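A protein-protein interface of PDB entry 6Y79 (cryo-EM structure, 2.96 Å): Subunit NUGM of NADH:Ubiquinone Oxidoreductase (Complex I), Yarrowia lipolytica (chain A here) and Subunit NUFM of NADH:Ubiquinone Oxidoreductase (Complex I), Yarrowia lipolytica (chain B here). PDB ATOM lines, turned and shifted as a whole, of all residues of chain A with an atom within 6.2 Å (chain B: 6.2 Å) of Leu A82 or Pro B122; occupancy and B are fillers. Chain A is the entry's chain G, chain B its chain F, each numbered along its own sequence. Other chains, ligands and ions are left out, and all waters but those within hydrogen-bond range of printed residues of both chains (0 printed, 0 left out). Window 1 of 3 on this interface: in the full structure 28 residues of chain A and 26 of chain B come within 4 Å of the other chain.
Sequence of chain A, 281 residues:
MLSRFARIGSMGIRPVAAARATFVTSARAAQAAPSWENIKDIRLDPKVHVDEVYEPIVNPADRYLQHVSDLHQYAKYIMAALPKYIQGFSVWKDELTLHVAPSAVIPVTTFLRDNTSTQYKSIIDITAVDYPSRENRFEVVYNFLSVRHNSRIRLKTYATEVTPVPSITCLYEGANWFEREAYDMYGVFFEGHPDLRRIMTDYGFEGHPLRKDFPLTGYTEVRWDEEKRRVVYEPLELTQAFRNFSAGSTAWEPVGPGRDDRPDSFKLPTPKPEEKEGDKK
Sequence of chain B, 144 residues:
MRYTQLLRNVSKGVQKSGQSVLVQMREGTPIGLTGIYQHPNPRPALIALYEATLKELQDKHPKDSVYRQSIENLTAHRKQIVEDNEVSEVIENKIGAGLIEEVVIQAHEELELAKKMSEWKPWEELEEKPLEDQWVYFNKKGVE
The backbone carbonyl oxygen of Pro B122 lies within hydrogen-bond range of the backbone NH of Lys A84. The backbone carbonyl oxygen of Trp B120 is in hydrogen-bond range of the side-chain amino group of Lys A84 (3.2 Å). OE1 of Glu B124 is in salt-bridge range of NZ of Lys A84, 3.6 Å away. The backbone carbonyl oxygen (O) of Trp B120 lies within hydrogen-bond range of the side-chain hydroxyl (OH) of Tyr A85, 3.2 Å away.
The side-chain amino group (NZ) of Lys A84 sits at hydrogen-bond distance from the side-chain hydroxyl (OH) of Tyr A85 (3.1 Å).
Tyr B67 touches Ala A81 (CB to O, 3.8 Å). Pro B122 touches Leu A82 (CB to CD2, 3.8 Å). Pro A83 touches Pro B122 (CD to O, 3.2 Å). Pro A83 touches Trp B123. Pro A83 touches Glu B124 (C to O, 3.6 Å). Lys B121 touches Lys A84. Lys A84 touches Glu B125. Tyr A85 touches Pro B122. CA of Pro A107 touches CZ3 of Trp B120, at 3.8 Å. Tyr B67 touches Phe A111.
Leu A82 touches one residue of chain B. Pro B122 touches four residues of chain A. Of the printed residues of chain A, Tyr B67 touches Ala A81 and Phe A111. Of the printed residues of chain B, Tyr A85 touches Trp B120 and Pro B122. Tyr A77 touches none of the printed residues of chain B. Ile A86 touches none of the printed residues of chain B.
Among the printed residues, Asp or Glu carboxylates within 4 Å of a Lys or Arg side-chain nitrogen of the other chain: Lys A84 with Glu B124.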
ATOM      1  N   TYR A  77      29.825 -17.852  26.976  1.00  0.00           N
ATOM      2  CA  TYR A  77      30.357 -19.080  27.527  1.00  0.00           C
ATOM      3  C   TYR A  77      29.246 -20.080  27.811  1.00  0.00           C
ATOM      4  O   TYR A  77      29.381 -21.263  27.481  1.00  0.00           O
ATOM      5  CB  TYR A  77      31.153 -18.796  28.790  1.00  0.00           C
ATOM      6  CG  TYR A  77      31.507 -20.076  29.457  1.00  0.00           C
ATOM      7  CD1 TYR A  77      32.389 -20.956  28.853  1.00  0.00           C
ATOM      8  CD2 TYR A  77      30.930 -20.434  30.664  1.00  0.00           C
ATOM      9  CE1 TYR A  77      32.695 -22.146  29.436  1.00  0.00           C
ATOM     10  CE2 TYR A  77      31.224 -21.617  31.249  1.00  0.00           C
ATOM     11  CZ  TYR A  77      32.105 -22.465  30.638  1.00  0.00           C
ATOM     12  OH  TYR A  77      32.373 -23.643  31.259  1.00  0.00           O
ATOM     13  N   ILE A  78      28.138 -19.618  28.403  1.00  0.00           N
ATOM     14  CA  ILE A  78      27.126 -20.535  28.927  1.00  0.00           C
ATOM     15  C   ILE A  78      26.437 -21.269  27.787  1.00  0.00           C
ATOM     16  O   ILE A  78      26.234 -22.488  27.849  1.00  0.00           O
ATOM     17  CB  ILE A  78      26.119 -19.776  29.812  1.00  0.00           C
ATOM     18  CG1 ILE A  78      26.822 -19.103  30.987  1.00  0.00           C
ATOM     19  CG2 ILE A  78      25.067 -20.701  30.360  1.00  0.00           C
ATOM     20  CD1 ILE A  78      27.433 -20.059  31.967  1.00  0.00           C
ATOM     21  N   MET A  79      26.146 -20.551  26.698  1.00  0.00           N
ATOM     22  CA  MET A  79      25.623 -21.171  25.486  1.00  0.00           C
ATOM     23  C   MET A  79      26.609 -22.173  24.904  1.00  0.00           C
ATOM     24  O   MET A  79      26.205 -23.235  24.417  1.00  0.00           O
ATOM     25  CB  MET A  79      25.296 -20.102  24.448  1.00  0.00           C
ATOM     26  CG  MET A  79      24.683 -20.666  23.196  1.00  0.00           C
ATOM     27  SD  MET A  79      24.431 -19.434  21.936  1.00  0.00           S
ATOM     28  CE  MET A  79      22.864 -18.796  22.446  1.00  0.00           C
ATOM     29  N   ALA A  80      27.906 -21.872  24.975  1.00  0.00           N
ATOM     30  CA  ALA A  80      28.893 -22.833  24.510  1.00  0.00           C
ATOM     31  C   ALA A  80      29.013 -24.027  25.441  1.00  0.00           C
ATOM     32  O   ALA A  80      29.430 -25.097  24.996  1.00  0.00           O
ATOM     33  CB  ALA A  80      30.250 -22.160  24.348  1.00  0.00           C
ATOM     34  N   ALA A  81      28.634 -23.881  26.714  1.00  0.00           N
ATOM     35  CA  ALA A  81      28.773 -25.003  27.632  1.00  0.00           C
ATOM     36  C   ALA A  81      27.599 -25.961  27.513  1.00  0.00           C
ATOM     37  O   ALA A  81      27.778 -27.176  27.628  1.00  0.00           O
ATOM     38  CB  ALA A  81      28.917 -24.504  29.068  1.00  0.00           C
ATOM     39  N   LEU A  82      26.395 -25.442  27.272  1.00  0.00           N
ATOM     40  CA  LEU A  82      25.199 -26.256  27.065  1.00  0.00           C
ATOM     41  C   LEU A  82      24.584 -25.952  25.703  1.00  0.00           C
ATOM     42  O   LEU A  82      23.561 -25.258  25.630  1.00  0.00           O
ATOM     43  CB  LEU A  82      24.160 -26.001  28.153  1.00  0.00           C
ATOM     44  CG  LEU A  82      24.510 -26.113  29.629  1.00  0.00           C
ATOM     45  CD1 LEU A  82      23.302 -25.718  30.439  1.00  0.00           C
ATOM     46  CD2 LEU A  82      24.925 -27.522  29.963  1.00  0.00           C
ATOM     47  N   PRO A  83      25.158 -26.459  24.605  1.00  0.00           N
ATOM     48  CA  PRO A  83      24.551 -26.206  23.292  1.00  0.00           C
ATOM     49  C   PRO A  83      23.256 -26.957  23.047  1.00  0.00           C
ATOM     50  O   PRO A  83      22.490 -26.554  22.169  1.00  0.00           O
ATOM     51  CB  PRO A  83      25.640 -26.659  22.317  1.00  0.00           C
ATOM     52  CG  PRO A  83      26.416 -27.632  23.065  1.00  0.00           C
ATOM     53  CD  PRO A  83      26.468 -27.111  24.449  1.00  0.00           C
ATOM     54  N   LYS A  84      22.990 -28.034  23.778  1.00  0.00           N
ATOM     55  CA  LYS A  84      21.767 -28.794  23.583  1.00  0.00           C
ATOM     56  C   LYS A  84      20.542 -28.091  24.156  1.00  0.00           C
ATOM     57  O   LYS A  84      19.413 -28.420  23.781  1.00  0.00           O
ATOM     58  CB  LYS A  84      21.915 -30.175  24.228  1.00  0.00           C
ATOM     59  CG  LYS A  84      20.938 -31.236  23.758  1.00  0.00           C
ATOM     60  CD  LYS A  84      20.969 -32.451  24.654  1.00  0.00           C
ATOM     61  CE  LYS A  84      19.676 -33.239  24.554  1.00  0.00           C
ATOM     62  NZ  LYS A  84      19.713 -34.469  25.385  1.00  0.00           N
ATOM     63  N   TYR A  85      20.727 -27.125  25.051  1.00  0.00           N
ATOM     64  CA  TYR A  85      19.615 -26.676  25.866  1.00  0.00           C
ATOM     65  C   TYR A  85      19.335 -25.175  25.845  1.00  0.00           C
ATOM     66  O   TYR A  85      18.249 -24.779  26.299  1.00  0.00           O
ATOM     67  CB  TYR A  85      19.824 -27.134  27.316  1.00  0.00           C
ATOM     68  CG  TYR A  85      19.761 -28.638  27.500  1.00  0.00           C
ATOM     69  CD1 TYR A  85      18.601 -29.339  27.216  1.00  0.00           C
ATOM     70  CD2 TYR A  85      20.856 -29.353  27.967  1.00  0.00           C
ATOM     71  CE1 TYR A  85      18.524 -30.699  27.381  1.00  0.00           C
ATOM     72  CE2 TYR A  85      20.791 -30.723  28.136  1.00  0.00           C
ATOM     73  CZ  TYR A  85      19.623 -31.387  27.840  1.00  0.00           C
ATOM     74  OH  TYR A  85      19.547 -32.749  28.001  1.00  0.00           O
ATOM     75  N   ILE A  86      20.231 -24.339  25.305  1.00  0.00           N
ATOM     76  CA  ILE A  86      20.093 -22.883  25.377  1.00  0.00           C
ATOM     77  C   ILE A  86      19.840 -22.370  23.970  1.00  0.00           C
ATOM     78  O   ILE A  86      20.767 -22.251  23.177  1.00  0.00           O
ATOM     79  CB  ILE A  86      21.330 -22.209  25.988  1.00  0.00           C
ATOM     80  CG1 ILE A  86      21.500 -22.656  27.448  1.00  0.00           C
ATOM     81  CG2 ILE A  86      21.221 -20.706  25.988  1.00  0.00           C
ATOM     82  CD1 ILE A  86      22.847 -22.326  27.951  1.00  0.00           C
ATOM     83  N   PRO A 107      17.552 -29.612  33.084  1.00  0.00           N
ATOM     84  CA  PRO A 107      19.016 -29.601  32.915  1.00  0.00           C
ATOM     85  C   PRO A 107      19.681 -28.233  32.977  1.00  0.00           C
ATOM     86  O   PRO A 107      20.877 -28.173  33.276  1.00  0.00           O
ATOM     87  CB  PRO A 107      19.208 -30.242  31.533  1.00  0.00           C
ATOM     88  CG  PRO A 107      17.884 -30.219  30.908  1.00  0.00           C
ATOM     89  CD  PRO A 107      16.964 -30.448  32.023  1.00  0.00           C
ATOM     90  N   VAL A 108      18.975 -27.134  32.704  1.00  0.00           N
ATOM     91  CA  VAL A 108      19.644 -25.836  32.756  1.00  0.00           C
ATOM     92  C   VAL A 108      19.696 -25.306  34.181  1.00  0.00           C
ATOM     93  O   VAL A 108      20.765 -24.890  34.648  1.00  0.00           O
ATOM     94  CB  VAL A 108      18.979 -24.835  31.795  1.00  0.00           C
ATOM     95  CG1 VAL A 108      19.507 -23.433  32.024  1.00  0.00           C
ATOM     96  CG2 VAL A 108      19.274 -25.222  30.388  1.00  0.00           C
ATOM     97  N   PHE A 111      22.256 -26.918  36.248  1.00  0.00           N
ATOM     98  CA  PHE A 111      23.539 -26.300  35.935  1.00  0.00           C
ATOM     99  C   PHE A 111      23.702 -24.972  36.662  1.00  0.00           C
ATOM    100  O   PHE A 111      24.710 -24.748  37.345  1.00  0.00           O
ATOM    101  CB  PHE A 111      23.656 -26.108  34.428  1.00  0.00           C
ATOM    102  CG  PHE A 111      24.942 -25.494  33.996  1.00  0.00           C
ATOM    103  CD1 PHE A 111      26.113 -26.225  34.021  1.00  0.00           C
ATOM    104  CD2 PHE A 111      24.981 -24.185  33.553  1.00  0.00           C
ATOM    105  CE1 PHE A 111      27.298 -25.659  33.618  1.00  0.00           C
ATOM    106  CE2 PHE A 111      26.162 -23.618  33.146  1.00  0.00           C
ATOM    107  CZ  PHE A 111      27.322 -24.356  33.180  1.00  0.00           C
ATOM    108  N   HIS B  61      33.067 -37.577  29.391  1.00  0.00           N
ATOM    109  CA  HIS B  61      32.734 -36.453  28.532  1.00  0.00           C
ATOM    110  C   HIS B  61      33.684 -36.389  27.339  1.00  0.00           C
ATOM    111  O   HIS B  61      34.858 -36.744  27.465  1.00  0.00           O
ATOM    112  CB  HIS B  61      32.798 -35.128  29.304  1.00  0.00           C
ATOM    113  CG  HIS B  61      31.731 -34.969  30.342  1.00  0.00           C
ATOM    114  ND1 HIS B  61      30.427 -34.651  30.031  1.00  0.00           N
ATOM    115  CD2 HIS B  61      31.779 -35.075  31.691  1.00  0.00           C
ATOM    116  CE1 HIS B  61      29.719 -34.573  31.142  1.00  0.00           C
ATOM    117  NE2 HIS B  61      30.514 -34.829  32.163  1.00  0.00           N
ATOM    118  N   TYR B  67      32.396 -27.489  28.154  1.00  0.00           N
ATOM    119  CA  TYR B  67      32.067 -27.822  29.539  1.00  0.00           C
ATOM    120  C   TYR B  67      33.178 -28.630  30.205  1.00  0.00           C
ATOM    121  O   TYR B  67      33.655 -28.282  31.299  1.00  0.00           O
ATOM    122  CB  TYR B  67      30.748 -28.599  29.546  1.00  0.00           C
ATOM    123  CG  TYR B  67      30.261 -29.031  30.896  1.00  0.00           C
ATOM    124  CD1 TYR B  67      29.556 -28.161  31.702  1.00  0.00           C
ATOM    125  CD2 TYR B  67      30.495 -30.317  31.359  1.00  0.00           C
ATOM    126  CE1 TYR B  67      29.103 -28.554  32.935  1.00  0.00           C
ATOM    127  CE2 TYR B  67      30.053 -30.715  32.595  1.00  0.00           C
ATOM    128  CZ  TYR B  67      29.357 -29.830  33.376  1.00  0.00           C
ATOM    129  OH  TYR B  67      28.916 -30.221  34.613  1.00  0.00           O
ATOM    130  N   MET B 117      25.589 -34.758  34.140  1.00  0.00           N
ATOM    131  CA  MET B 117      25.741 -34.256  32.778  1.00  0.00           C
ATOM    132  C   MET B 117      26.017 -35.348  31.751  1.00  0.00           C
ATOM    133  O   MET B 117      25.654 -35.180  30.586  1.00  0.00           O
ATOM    134  CB  MET B 117      26.863 -33.227  32.704  1.00  0.00           C
ATOM    135  CG  MET B 117      26.488 -31.861  33.211  1.00  0.00           C
ATOM    136  SD  MET B 117      25.071 -31.111  32.396  1.00  0.00           S
ATOM    137  CE  MET B 117      23.992 -30.884  33.797  1.00  0.00           C
ATOM    138  N   SER B 118      26.642 -36.457  32.139  1.00  0.00           N
ATOM    139  CA  SER B 118      26.870 -37.517  31.165  1.00  0.00           C
ATOM    140  C   SER B 118      25.621 -38.345  30.914  1.00  0.00           C
ATOM    141  O   SER B 118      25.517 -38.992  29.867  1.00  0.00           O
ATOM    142  CB  SER B 118      28.019 -38.408  31.618  1.00  0.00           C
ATOM    143  OG  SER B 118      29.215 -37.664  31.603  1.00  0.00           O
ATOM    144  N   TRP B 120      22.656 -36.659  30.927  1.00  0.00           N
ATOM    145  CA  TRP B 120      21.871 -35.723  30.126  1.00  0.00           C
ATOM    146  C   TRP B 120      22.486 -35.429  28.763  1.00  0.00           C
ATOM    147  O   TRP B 120      21.739 -35.135  27.823  1.00  0.00           O
ATOM    148  CB  TRP B 120      21.639 -34.427  30.911  1.00  0.00           C
ATOM    149  CG  TRP B 120      20.530 -34.589  31.904  1.00  0.00           C
ATOM    150  CD1 TRP B 120      19.517 -35.496  31.842  1.00  0.00           C
ATOM    151  CD2 TRP B 120      20.350 -33.873  33.131  1.00  0.00           C
ATOM    152  NE1 TRP B 120      18.692 -35.369  32.938  1.00  0.00           N
ATOM    153  CE2 TRP B 120      19.190 -34.382  33.746  1.00  0.00           C
ATOM    154  CE3 TRP B 120      21.049 -32.848  33.765  1.00  0.00           C
ATOM    155  CZ2 TRP B 120      18.721 -33.898  34.959  1.00  0.00           C
ATOM    156  CZ3 TRP B 120      20.584 -32.372  34.969  1.00  0.00           C
ATOM    157  CH2 TRP B 120      19.432 -32.896  35.552  1.00  0.00           C
ATOM    158  N   LYS B 121      23.815 -35.542  28.633  1.00  0.00           N
ATOM    159  CA  LYS B 121      24.615 -35.346  27.420  1.00  0.00           C
ATOM    160  C   LYS B 121      24.332 -34.010  26.743  1.00  0.00           C
ATOM    161  O   LYS B 121      23.725 -33.991  25.667  1.00  0.00           O
ATOM    162  CB  LYS B 121      24.371 -36.474  26.411  1.00  0.00           C
ATOM    163  CG  LYS B 121      24.933 -37.835  26.780  1.00  0.00           C
ATOM    164  CD  LYS B 121      24.644 -38.846  25.678  1.00  0.00           C
ATOM    165  CE  LYS B 121      24.984 -40.261  26.107  1.00  0.00           C
ATOM    166  NZ  LYS B 121      24.712 -41.259  25.034  1.00  0.00           N
ATOM    167  N   PRO B 122      24.745 -32.879  27.312  1.00  0.00           N
ATOM    168  CA  PRO B 122      24.366 -31.586  26.742  1.00  0.00           C
ATOM    169  C   PRO B 122      25.280 -31.051  25.651  1.00  0.00           C
ATOM    170  O   PRO B 122      25.069 -29.917  25.221  1.00  0.00           O
ATOM    171  CB  PRO B 122      24.414 -30.675  27.970  1.00  0.00           C
ATOM    172  CG  PRO B 122      25.511 -31.215  28.758  1.00  0.00           C
ATOM    173  CD  PRO B 122      25.526 -32.699  28.546  1.00  0.00           C
ATOM    174  N   TRP B 123      26.267 -31.808  25.177  1.00  0.00           N
ATOM    175  CA  TRP B 123      27.085 -31.331  24.068  1.00  0.00           C
ATOM    176  C   TRP B 123      26.450 -31.581  22.708  1.00  0.00           C
ATOM    177  O   TRP B 123      27.072 -31.271  21.691  1.00  0.00           O
ATOM    178  CB  TRP B 123      28.474 -31.974  24.100  1.00  0.00           C
ATOM    179  CG  TRP B 123      28.448 -33.461  23.978  1.00  0.00           C
ATOM    180  CD1 TRP B 123      28.445 -34.195  22.826  1.00  0.00           C
ATOM    181  CD2 TRP B 123      28.426 -34.401  25.052  1.00  0.00           C
ATOM    182  NE1 TRP B 123      28.412 -35.532  23.118  1.00  0.00           N
ATOM    183  CE2 TRP B 123      28.398 -35.686  24.479  1.00  0.00           C
ATOM    184  CE3 TRP B 123      28.423 -34.282  26.442  1.00  0.00           C
ATOM    185  CZ2 TRP B 123      28.376 -36.842  25.249  1.00  0.00           C
ATOM    186  CZ3 TRP B 123      28.396 -35.429  27.204  1.00  0.00           C
ATOM    187  CH2 TRP B 123      28.374 -36.692  26.608  1.00  0.00           C
ATOM    188  N   GLU B 124      25.248 -32.149  22.661  1.00  0.00           N
ATOM    189  CA  GLU B 124      24.583 -32.410  21.397  1.00  0.00           C
ATOM    190  C   GLU B 124      24.046 -31.115  20.791  1.00  0.00           C
ATOM    191  O   GLU B 124      24.089 -30.047  21.398  1.00  0.00           O
ATOM    192  CB  GLU B 124      23.431 -33.395  21.592  1.00  0.00           C
ATOM    193  CG  GLU B 124      23.811 -34.725  22.219  1.00  0.00           C
ATOM    194  CD  GLU B 124      22.601 -35.617  22.443  1.00  0.00           C
ATOM    195  OE1 GLU B 124      21.463 -35.110  22.358  1.00  0.00           O
ATOM    196  OE2 GLU B 124      22.781 -36.826  22.695  1.00  0.00           O
ATOM    197  N   GLU B 125      23.534 -31.225  19.571  1.00  0.00           N
ATOM    198  CA  GLU B 125      22.712 -30.165  19.010  1.00  0.00           C
ATOM    199  C   GLU B 125      21.399 -30.075  19.782  1.00  0.00           C
ATOM    200  O   GLU B 125      20.968 -31.035  20.426  1.00  0.00           O
ATOM    201  CB  GLU B 125      22.434 -30.433  17.532  1.00  0.00           C
ATOM    202  CG  GLU B 125      23.674 -30.481  16.666  1.00  0.00           C
ATOM    203  CD  GLU B 125      24.239 -29.105  16.400  1.00  0.00           C
ATOM    204  OE1 GLU B 125      23.451 -28.138  16.364  1.00  0.00           O
ATOM    205  OE2 GLU B 125      25.465 -28.988  16.220  1.00  0.00           O
